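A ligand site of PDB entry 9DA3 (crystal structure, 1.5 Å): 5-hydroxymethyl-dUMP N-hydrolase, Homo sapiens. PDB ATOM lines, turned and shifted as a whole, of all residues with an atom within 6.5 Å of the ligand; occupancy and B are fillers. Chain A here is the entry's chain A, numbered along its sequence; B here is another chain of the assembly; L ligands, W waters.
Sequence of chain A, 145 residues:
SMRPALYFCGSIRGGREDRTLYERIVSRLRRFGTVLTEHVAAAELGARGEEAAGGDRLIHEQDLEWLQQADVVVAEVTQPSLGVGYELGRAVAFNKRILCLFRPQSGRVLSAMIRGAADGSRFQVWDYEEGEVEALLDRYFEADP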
ATOM      1  N   TYR A   7     -31.686  13.852   0.061  1.00  0.00           N
ATOM      2  CA  TYR A   7     -31.517  15.285  -0.107  1.00  0.00           C
ATOM      3  C   TYR A   7     -30.013  15.525  -0.146  1.00  0.00           C
ATOM      4  O   TYR A   7     -29.310  15.158   0.804  1.00  0.00           O
ATOM      5  CB  TYR A   7     -32.106  16.050   1.081  1.00  0.00           C
ATOM      6  CG  TYR A   7     -32.182  17.539   0.893  1.00  0.00           C
ATOM      7  CD1 TYR A   7     -31.066  18.340   1.116  1.00  0.00           C
ATOM      8  CD2 TYR A   7     -33.407  18.162   0.715  1.00  0.00           C
ATOM      9  CE1 TYR A   7     -31.146  19.703   0.989  1.00  0.00           C
ATOM     10  CE2 TYR A   7     -33.513  19.524   0.612  1.00  0.00           C
ATOM     11  CZ  TYR A   7     -32.362  20.288   0.743  1.00  0.00           C
ATOM     12  OH  TYR A   7     -32.439  21.663   0.660  1.00  0.00           O
ATOM     13  N   PHE A   8     -29.503  16.135  -1.218  1.00  0.00           N
ATOM     14  CA  PHE A   8     -28.073  16.426  -1.308  1.00  0.00           C
ATOM     15  C   PHE A   8     -27.776  17.914  -1.120  1.00  0.00           C
ATOM     16  O   PHE A   8     -28.442  18.768  -1.714  1.00  0.00           O
ATOM     17  CB  PHE A   8     -27.487  15.981  -2.651  1.00  0.00           C
ATOM     18  CG  PHE A   8     -26.045  16.376  -2.804  1.00  0.00           C
ATOM     19  CD1 PHE A   8     -25.061  15.705  -2.098  1.00  0.00           C
ATOM     20  CD2 PHE A   8     -25.698  17.504  -3.544  1.00  0.00           C
ATOM     21  CE1 PHE A   8     -23.729  16.108  -2.172  1.00  0.00           C
ATOM     22  CE2 PHE A   8     -24.372  17.910  -3.631  1.00  0.00           C
ATOM     23  CZ  PHE A   8     -23.390  17.202  -2.942  1.00  0.00           C
ATOM     24  N   CYS A   9     -26.724  18.207  -0.343  1.00  0.00           N
ATOM     25  CA  CYS A   9     -26.273  19.580  -0.094  1.00  0.00           C
ATOM     26  C   CYS A   9     -24.820  19.769  -0.553  1.00  0.00           C
ATOM     27  O   CYS A   9     -23.945  18.987  -0.186  1.00  0.00           O
ATOM     28  CB  CYS A   9     -26.335  19.983   1.383  1.00  0.00           C
ATOM     29  SG  CYS A   9     -27.764  19.431   2.338  1.00  0.00           S
ATOM     30  N   GLY A  10     -24.570  20.850  -1.305  1.00  0.00           N
ATOM     31  CA  GLY A  10     -23.226  21.214  -1.697  1.00  0.00           C
ATOM     32  C   GLY A  10     -23.218  22.666  -2.153  1.00  0.00           C
ATOM     33  O   GLY A  10     -24.192  23.153  -2.722  1.00  0.00           O
ATOM     34  N   SER A  11     -22.111  23.354  -1.879  1.00  0.00           N
ATOM     35  CA  SER A  11     -21.983  24.782  -2.194  1.00  0.00           C
ATOM     36  C   SER A  11     -22.347  25.094  -3.633  1.00  0.00           C
ATOM     37  O   SER A  11     -21.924  24.402  -4.578  1.00  0.00           O
ATOM     38  CB  SER A  11     -20.542  25.225  -1.931  1.00  0.00           C
ATOM     39  OG  SER A  11     -20.353  26.619  -2.173  1.00  0.00           O
ATOM     40  N   ILE A  12     -23.095  26.201  -3.805  1.00  0.00           N
ATOM     41  CA  ILE A  12     -23.359  26.756  -5.135  1.00  0.00           C
ATOM     42  C   ILE A  12     -22.903  28.218  -5.120  1.00  0.00           C
ATOM     43  O   ILE A  12     -21.832  28.537  -5.673  1.00  0.00           O
ATOM     44  CB  ILE A  12     -24.842  26.614  -5.534  1.00  0.00           C
ATOM     45  CG1 ILE A  12     -25.228  25.124  -5.557  1.00  0.00           C
ATOM     46  CG2 ILE A  12     -25.085  27.271  -6.924  1.00  0.00           C
ATOM     47  CD1 ILE A  12     -26.709  24.879  -5.858  1.00  0.00           C
ATOM     48  N   ARG A  13     -23.661  29.107  -4.476  1.00  0.00           N
ATOM     49  CA  ARG A  13     -23.199  30.496  -4.410  1.00  0.00           C
ATOM     50  C   ARG A  13     -22.004  30.668  -3.482  1.00  0.00           C
ATOM     51  O   ARG A  13     -21.275  31.654  -3.618  1.00  0.00           O
ATOM     52  CB  ARG A  13     -24.350  31.426  -4.025  1.00  0.00           C
ATOM     53  CG  ARG A  13     -25.443  31.415  -5.098  1.00  0.00           C
ATOM     54  CD  ARG A  13     -26.522  32.397  -4.811  1.00  0.00           C
ATOM     55  NE  ARG A  13     -27.591  32.325  -5.804  1.00  0.00           N
ATOM     56  CZ  ARG A  13     -28.803  32.856  -5.641  1.00  0.00           C
ATOM     57  NH1 ARG A  13     -29.099  33.591  -4.583  1.00  0.00           N
ATOM     58  NH2 ARG A  13     -29.745  32.607  -6.550  1.00  0.00           N
ATOM     59  N   GLY A  14     -21.741  29.712  -2.600  1.00  0.00           N
ATOM     60  CA  GLY A  14     -20.464  29.767  -1.902  1.00  0.00           C
ATOM     61  C   GLY A  14     -19.273  29.450  -2.787  1.00  0.00           C
ATOM     62  O   GLY A  14     -18.133  29.672  -2.366  1.00  0.00           O
ATOM     63  N   GLY A  15     -19.518  28.982  -4.008  1.00  0.00           N
ATOM     64  CA  GLY A  15     -18.470  28.576  -4.923  1.00  0.00           C
ATOM     65  C   GLY A  15     -18.740  27.184  -5.443  1.00  0.00           C
ATOM     66  O   GLY A  15     -19.210  26.318  -4.699  1.00  0.00           O
ATOM     67  N   THR A  37     -33.523  16.751  -4.436  1.00  0.00           N
ATOM     68  CA  THR A  37     -32.992  18.072  -4.730  1.00  0.00           C
ATOM     69  C   THR A  37     -32.568  18.236  -6.184  1.00  0.00           C
ATOM     70  O   THR A  37     -32.185  19.341  -6.585  1.00  0.00           O
ATOM     71  CB  THR A  37     -31.804  18.371  -3.813  1.00  0.00           C
ATOM     72  OG1 THR A  37     -30.972  17.202  -3.693  1.00  0.00           O
ATOM     73  CG2 THR A  37     -32.302  18.705  -2.437  1.00  0.00           C
ATOM     74  N   ASP A  56     -35.451  33.615  -5.009  1.00  0.00           N
ATOM     75  CA  ASP A  56     -34.820  32.836  -3.961  1.00  0.00           C
ATOM     76  C   ASP A  56     -35.820  32.320  -2.943  1.00  0.00           C
ATOM     77  O   ASP A  56     -35.559  31.298  -2.292  1.00  0.00           O
ATOM     78  CB  ASP A  56     -33.740  33.668  -3.271  1.00  0.00           C
ATOM     79  CG  ASP A  56     -32.557  33.933  -4.182  1.00  0.00           C
ATOM     80  OD1 ASP A  56     -32.430  33.259  -5.230  1.00  0.00           O
ATOM     81  OD2 ASP A  56     -31.694  34.742  -3.791  1.00  0.00           O
ATOM     82  N   ILE A  59     -36.857  28.868  -4.080  1.00  0.00           N
ATOM     83  CA  ILE A  59     -35.806  27.899  -3.765  1.00  0.00           C
ATOM     84  C   ILE A  59     -35.879  27.501  -2.294  1.00  0.00           C
ATOM     85  O   ILE A  59     -35.889  26.320  -1.948  1.00  0.00           O
ATOM     86  CB  ILE A  59     -34.423  28.477  -4.120  1.00  0.00           C
ATOM     87  CG1 ILE A  59     -34.300  28.673  -5.645  1.00  0.00           C
ATOM     88  CG2 ILE A  59     -33.314  27.615  -3.562  1.00  0.00           C
ATOM     89  CD1 ILE A  59     -33.123  29.538  -6.065  1.00  0.00           C
ATOM     90  N   HIS A  60     -35.989  28.494  -1.405  1.00  0.00           N
ATOM     91  CA  HIS A  60     -35.996  28.189   0.025  1.00  0.00           C
ATOM     92  C   HIS A  60     -37.202  27.329   0.397  1.00  0.00           C
ATOM     93  O   HIS A  60     -37.063  26.306   1.079  1.00  0.00           O
ATOM     94  CB  HIS A  60     -36.008  29.499   0.815  1.00  0.00           C
ATOM     95  CG  HIS A  60     -36.102  29.306   2.306  1.00  0.00           C
ATOM     96  ND1 HIS A  60     -37.308  29.188   2.965  1.00  0.00           N
ATOM     97  CD2 HIS A  60     -35.135  29.196   3.242  1.00  0.00           C
ATOM     98  CE1 HIS A  60     -37.065  29.013   4.261  1.00  0.00           C
ATOM     99  NE2 HIS A  60     -35.755  29.016   4.445  1.00  0.00           N
ATOM    100  N   ASP A  63     -37.071  23.778  -1.122  1.00  0.00           N
ATOM    101  CA  ASP A  63     -36.064  22.928  -0.514  1.00  0.00           C
ATOM    102  C   ASP A  63     -36.446  22.548   0.913  1.00  0.00           C
ATOM    103  O   ASP A  63     -36.154  21.442   1.358  1.00  0.00           O
ATOM    104  CB  ASP A  63     -34.710  23.628  -0.594  1.00  0.00           C
ATOM    105  CG  ASP A  63     -34.018  23.360  -1.910  1.00  0.00           C
ATOM    106  OD1 ASP A  63     -33.902  24.297  -2.732  1.00  0.00           O
ATOM    107  OD2 ASP A  63     -33.600  22.215  -2.151  1.00  0.00           O
ATOM    108  N   PRO A  80     -16.918  26.049   2.077  1.00  0.00           N
ATOM    109  CA  PRO A  80     -17.827  26.794   2.961  1.00  0.00           C
ATOM    110  C   PRO A  80     -18.985  27.434   2.216  1.00  0.00           C
ATOM    111  O   PRO A  80     -18.823  28.007   1.133  1.00  0.00           O
ATOM    112  CB  PRO A  80     -16.914  27.855   3.596  1.00  0.00           C
ATOM    113  CG  PRO A  80     -15.549  27.209   3.545  1.00  0.00           C
ATOM    114  CD  PRO A  80     -15.515  26.480   2.223  1.00  0.00           C
ATOM    115  N   SER A  81     -20.172  27.355   2.823  1.00  0.00           N
ATOM    116  CA  SER A  81     -21.395  27.772   2.149  1.00  0.00           C
ATOM    117  C   SER A  81     -22.459  28.070   3.198  1.00  0.00           C
ATOM    118  O   SER A  81     -22.722  27.218   4.049  1.00  0.00           O
ATOM    119  CB  SER A  81     -21.880  26.664   1.184  1.00  0.00           C
ATOM    120  OG  SER A  81     -23.276  26.816   0.900  1.00  0.00           O
ATOM    121  N   LEU A  82     -23.059  29.253   3.117  1.00  0.00           N
ATOM    122  CA  LEU A  82     -24.181  29.568   4.019  1.00  0.00           C
ATOM    123  C   LEU A  82     -25.355  28.646   3.771  1.00  0.00           C
ATOM    124  O   LEU A  82     -26.006  28.203   4.722  1.00  0.00           O
ATOM    125  CB  LEU A  82     -24.627  31.013   3.824  1.00  0.00           C
ATOM    126  CG  LEU A  82     -23.610  32.110   4.116  1.00  0.00           C
ATOM    127  CD1 LEU A  82     -24.131  33.371   3.462  1.00  0.00           C
ATOM    128  CD2 LEU A  82     -23.427  32.306   5.598  1.00  0.00           C
ATOM    129  N   GLY A  83     -25.651  28.368   2.508  1.00  0.00           N
ATOM    130  CA  GLY A  83     -26.822  27.562   2.197  1.00  0.00           C
ATOM    131  C   GLY A  83     -26.699  26.137   2.691  1.00  0.00           C
ATOM    132  O   GLY A  83     -27.660  25.566   3.206  1.00  0.00           O
ATOM    133  N   VAL A  84     -25.494  25.558   2.569  1.00  0.00           N
ATOM    134  CA  VAL A  84     -25.290  24.211   3.086  1.00  0.00           C
ATOM    135  C   VAL A  84     -25.411  24.210   4.614  1.00  0.00           C
ATOM    136  O   VAL A  84     -26.063  23.348   5.198  1.00  0.00           O
ATOM    137  CB  VAL A  84     -23.922  23.669   2.635  1.00  0.00           C
ATOM    138  CG1 VAL A  84     -23.621  22.326   3.324  1.00  0.00           C
ATOM    139  CG2 VAL A  84     -23.896  23.530   1.101  1.00  0.00           C
ATOM    140  N   GLU A  87     -29.133  24.531   5.530  1.00  0.00           N
ATOM    141  CA  GLU A  87     -29.801  23.252   5.306  1.00  0.00           C
ATOM    142  C   GLU A  87     -29.525  22.273   6.439  1.00  0.00           C
ATOM    143  O   GLU A  87     -30.435  21.590   6.916  1.00  0.00           O
ATOM    144  CB  GLU A  87     -29.371  22.640   3.969  1.00  0.00           C
ATOM    145  CG  GLU A  87     -30.013  23.348   2.780  1.00  0.00           C
ATOM    146  CD  GLU A  87     -29.430  22.989   1.420  1.00  0.00           C
ATOM    147  OE1 GLU A  87     -28.216  22.706   1.301  1.00  0.00           O
ATOM    148  OE2 GLU A  87     -30.202  23.032   0.438  1.00  0.00           O
ATOM    149  N   VAL B 109     -23.162  37.041  -4.837  1.00  0.00           N
ATOM    150  CA  VAL B 109     -24.605  36.872  -4.832  1.00  0.00           C
ATOM    151  C   VAL B 109     -24.936  36.079  -3.580  1.00  0.00           C
ATOM    152  O   VAL B 109     -24.495  34.930  -3.418  1.00  0.00           O
ATOM    153  CB  VAL B 109     -25.100  36.166  -6.095  1.00  0.00           C
ATOM    154  CG1 VAL B 109     -26.612  36.061  -6.056  1.00  0.00           C
ATOM    155  CG2 VAL B 109     -24.626  36.889  -7.345  1.00  0.00           C
ATOM    156  N   LEU B 110     -25.669  36.700  -2.652  1.00  0.00           N
ATOM    157  CA  LEU B 110     -25.968  36.054  -1.386  1.00  0.00           C
ATOM    158  C   LEU B 110     -26.792  34.784  -1.607  1.00  0.00           C
ATOM    159  O   LEU B 110     -27.729  34.760  -2.412  1.00  0.00           O
ATOM    160  CB  LEU B 110     -26.747  37.001  -0.465  1.00  0.00           C
ATOM    161  CG  LEU B 110     -27.246  36.411   0.854  1.00  0.00           C
ATOM    162  CD1 LEU B 110     -26.104  35.972   1.735  1.00  0.00           C
ATOM    163  CD2 LEU B 110     -28.135  37.459   1.555  1.00  0.00           C
ATOM    164  N   SER B 111     -26.407  33.723  -0.889  1.00  0.00           N
ATOM    165  CA  SER B 111     -27.128  32.452  -0.823  1.00  0.00           C
ATOM    166  C   SER B 111     -28.637  32.602  -0.926  1.00  0.00           C
ATOM    167  O   SER B 111     -29.239  33.380  -0.189  1.00  0.00           O
ATOM    168  CB  SER B 111     -26.813  31.760   0.496  1.00  0.00           C
ATOM    169  OG  SER B 111     -27.474  30.499   0.579  1.00  0.00           O
ATOM    170  N   ALA B 112     -29.256  31.836  -1.822  1.00  0.00           N
ATOM    171  CA  ALA B 112     -30.716  31.821  -1.900  1.00  0.00           C
ATOM    172  C   ALA B 112     -31.354  31.356  -0.605  1.00  0.00           C
ATOM    173  O   ALA B 112     -32.509  31.710  -0.322  1.00  0.00           O
ATOM    174  CB  ALA B 112     -31.193  30.936  -3.054  1.00  0.00           C
ATOM    175  N   MET B 113     -30.631  30.545   0.189  1.00  0.00           N
ATOM    176  CA  MET B 113     -31.226  30.040   1.404  1.00  0.00           C
ATOM    177  C   MET B 113     -31.364  31.137   2.451  1.00  0.00           C
ATOM    178  O   MET B 113     -32.258  31.084   3.304  1.00  0.00           O
ATOM    179  CB  MET B 113     -30.385  28.883   1.958  1.00  0.00           C
ATOM    180  CG  MET B 113     -30.454  27.610   1.143  1.00  0.00           C
ATOM    181  SD  MET B 113     -32.047  27.120   0.499  1.00  0.00           S
ATOM    182  CE  MET B 113     -32.626  26.066   1.822  1.00  0.00           C
ATOM    183  N   ILE B 114     -30.490  32.125   2.415  1.00  0.00           N
ATOM    184  CA  ILE B 114     -30.586  33.217   3.366  1.00  0.00           C
ATOM    185  C   ILE B 114     -31.506  34.307   2.833  1.00  0.00           C
ATOM    186  O   ILE B 114     -32.434  34.755   3.524  1.00  0.00           O
ATOM    187  CB  ILE B 114     -29.181  33.757   3.678  1.00  0.00           C
ATOM    188  CG1 ILE B 114     -28.288  32.612   4.195  1.00  0.00           C
ATOM    189  CG2 ILE B 114     -29.257  34.908   4.676  1.00  0.00           C
ATOM    190  CD1 ILE B 114     -28.863  31.787   5.350  1.00  0.00           C
HETATM  191  C1  LIG L   1     -28.611  23.733  -2.532  1.00  0.00           C
HETATM  192  C2  LIG L   1     -29.490  27.232  -3.397  1.00  0.00           C
HETATM  193  C3  LIG L   1     -28.442  29.250  -4.590  1.00  0.00           C
HETATM  194  C4  LIG L   1     -27.227  23.549  -1.891  1.00  0.00           C
HETATM  195  C5  LIG L   1     -27.080  24.846  -0.989  1.00  0.00           C
HETATM  196  C6  LIG L   1     -26.088  25.861  -1.722  1.00  0.00           C
HETATM  197  C7  LIG L   1     -28.280  25.421  -0.846  1.00  0.00           C
HETATM  198  C8  LIG L   1     -30.498  25.200  -2.207  1.00  0.00           C
HETATM  199  C9  LIG L   1     -30.149  25.988  -3.498  1.00  0.00           C
HETATM  200  C10 LIG L   1     -30.488  25.477  -4.750  1.00  0.00           C
HETATM  201  C11 LIG L   1     -29.554  27.307  -5.764  1.00  0.00           C
HETATM  202  C12 LIG L   1     -29.177  27.898  -4.572  1.00  0.00           C
HETATM  203  N1  LIG L   1     -29.327  24.462  -1.643  1.00  0.00           N
HETATM  204  N2  LIG L   1     -30.181  26.139  -5.854  1.00  0.00           N
HETATM  205  O1  LIG L   1     -27.125  22.420  -1.121  1.00  0.00           O
HETATM  206  O2  LIG L   1     -26.070  27.018  -0.909  1.00  0.00           O
HETATM  207  O3  LIG L   1     -25.332  29.293  -0.273  1.00  0.00           O
HETATM  208  O4  LIG L   1     -23.756  27.840  -1.573  1.00  0.00           O
HETATM  209  O5  LIG L   1     -25.779  28.724  -2.724  1.00  0.00           O
HETATM  210  O6  LIG L   1     -29.238  27.957  -6.962  1.00  0.00           O
HETATM  211  O7  LIG L   1     -28.092  29.655  -3.280  1.00  0.00           O
HETATM  212  P1  LIG L   1     -25.192  28.293  -1.396  1.00  0.00           P
HETATM  213  O   HOH W   1     -27.829  30.367  -7.933  1.00  0.00           O
HETATM  214  O   HOH W   2     -30.115  20.968  -1.877  1.00  0.00           O
HETATM  215  O   HOH W   3     -23.086  30.690   0.611  1.00  0.00           O
HETATM  216  O   HOH W   4     -28.079  26.430  -9.342  1.00  0.00           O
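Merely in contact with the ligand: Cys 9 (3.1 Å), Ile 59 (3.6 Å), Asp 63 (3.6 Å), Ser 11 (3.6 Å), Met 113 of chain B (3.7 Å), Val 84 (3.8 Å) and Phe 8 (3.9 Å). Of the 26 residues printed, 16 come within 4 Å of the ligand.
The side-chain hydroxyl of Ser 111 of chain B lies within hydrogen-bond range of the backbone NH of Gly 83, at 3.4 Å. The backbone NH (N) of Met 113 of chain B sits close to the side-chain hydroxyl (OG) of Ser 111 of chain B, at 3.2 Å. The side-chain carboxylate (OE1) of Glu 87 sits close to the side-chain sulfur (SG) of Cys 9 (3.5 Å). The side-chain carboxylate (OE2) of Glu 87 lies within hydrogen-bond range of the side-chain hydroxyl (OH) of Tyr 7. The backbone carbonyl oxygen of Leu 110 of chain B sits at hydrogen-bond distance from the guanidinium group of Arg 13. The side-chain hydroxyl of Ser 11 sits close to the backbone NH of Gly 14, at 3.4 Å. OD2 of Asp 63 is in hydrogen-bond range of OH of Tyr 7 (3.1 Å). The side-chain hydroxyl (OG) of Ser 11 is in hydrogen-bond range of the backbone carbonyl oxygen (O) of Gly 15, at 2.8 Å.
Water W3 lies within hydrogen-bond range of O3 of the ligand (2.8 Å) and N of Leu 82 (2.9 Å). Water W1 bridges NE of Arg 13 (2.9 Å) and O6 of the ligand (3.0 Å). Water W2 lies within hydrogen-bond range of the backbone carbonyl oxygen (O) of Phe 8 (2.8 Å), the side-chain carboxylate (OE2) of Glu 87 (3.1 Å) and an oxygen (O1) of the ligand (3.4 Å).
An oxygen (O3) of the ligand sits at hydrogen-bond distance from the side-chain hydroxyl (OG) of Ser 111 of chain B, 2.6 Å away. A nitrogen (N1) of the ligand is in salt-bridge range of the side-chain carboxylate (OE2) of Glu 87 (2.7 Å). OG of Ser 81 lies within hydrogen-bond range of O4 of the ligand. The backbone NH (N) of Arg 13 lies within hydrogen-bond range of an oxygen (O5) of the ligand (2.8 Å). N of Ile 12 is in hydrogen-bond range of O4 of the ligand (2.8 Å). N of Ala 112 of chain B sits at hydrogen-bond distance from O7 of the ligand (2.9 Å). The backbone NH (N) of Gly 14 sits at hydrogen-bond distance from an oxygen (O4) of the ligand (2.9 Å). The backbone NH (N) of Gly 83 sits at hydrogen-bond distance from an oxygen (O3) of the ligand, at 2.9 Å. The backbone NH (N) of Gly 10 lies within hydrogen-bond range of an oxygen (O1) of the ligand, at 3.0 Å. The backbone carbonyl oxygen (O) of Gly 10 lies close to an oxygen (O1) of the ligand, at 3.4 Å.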
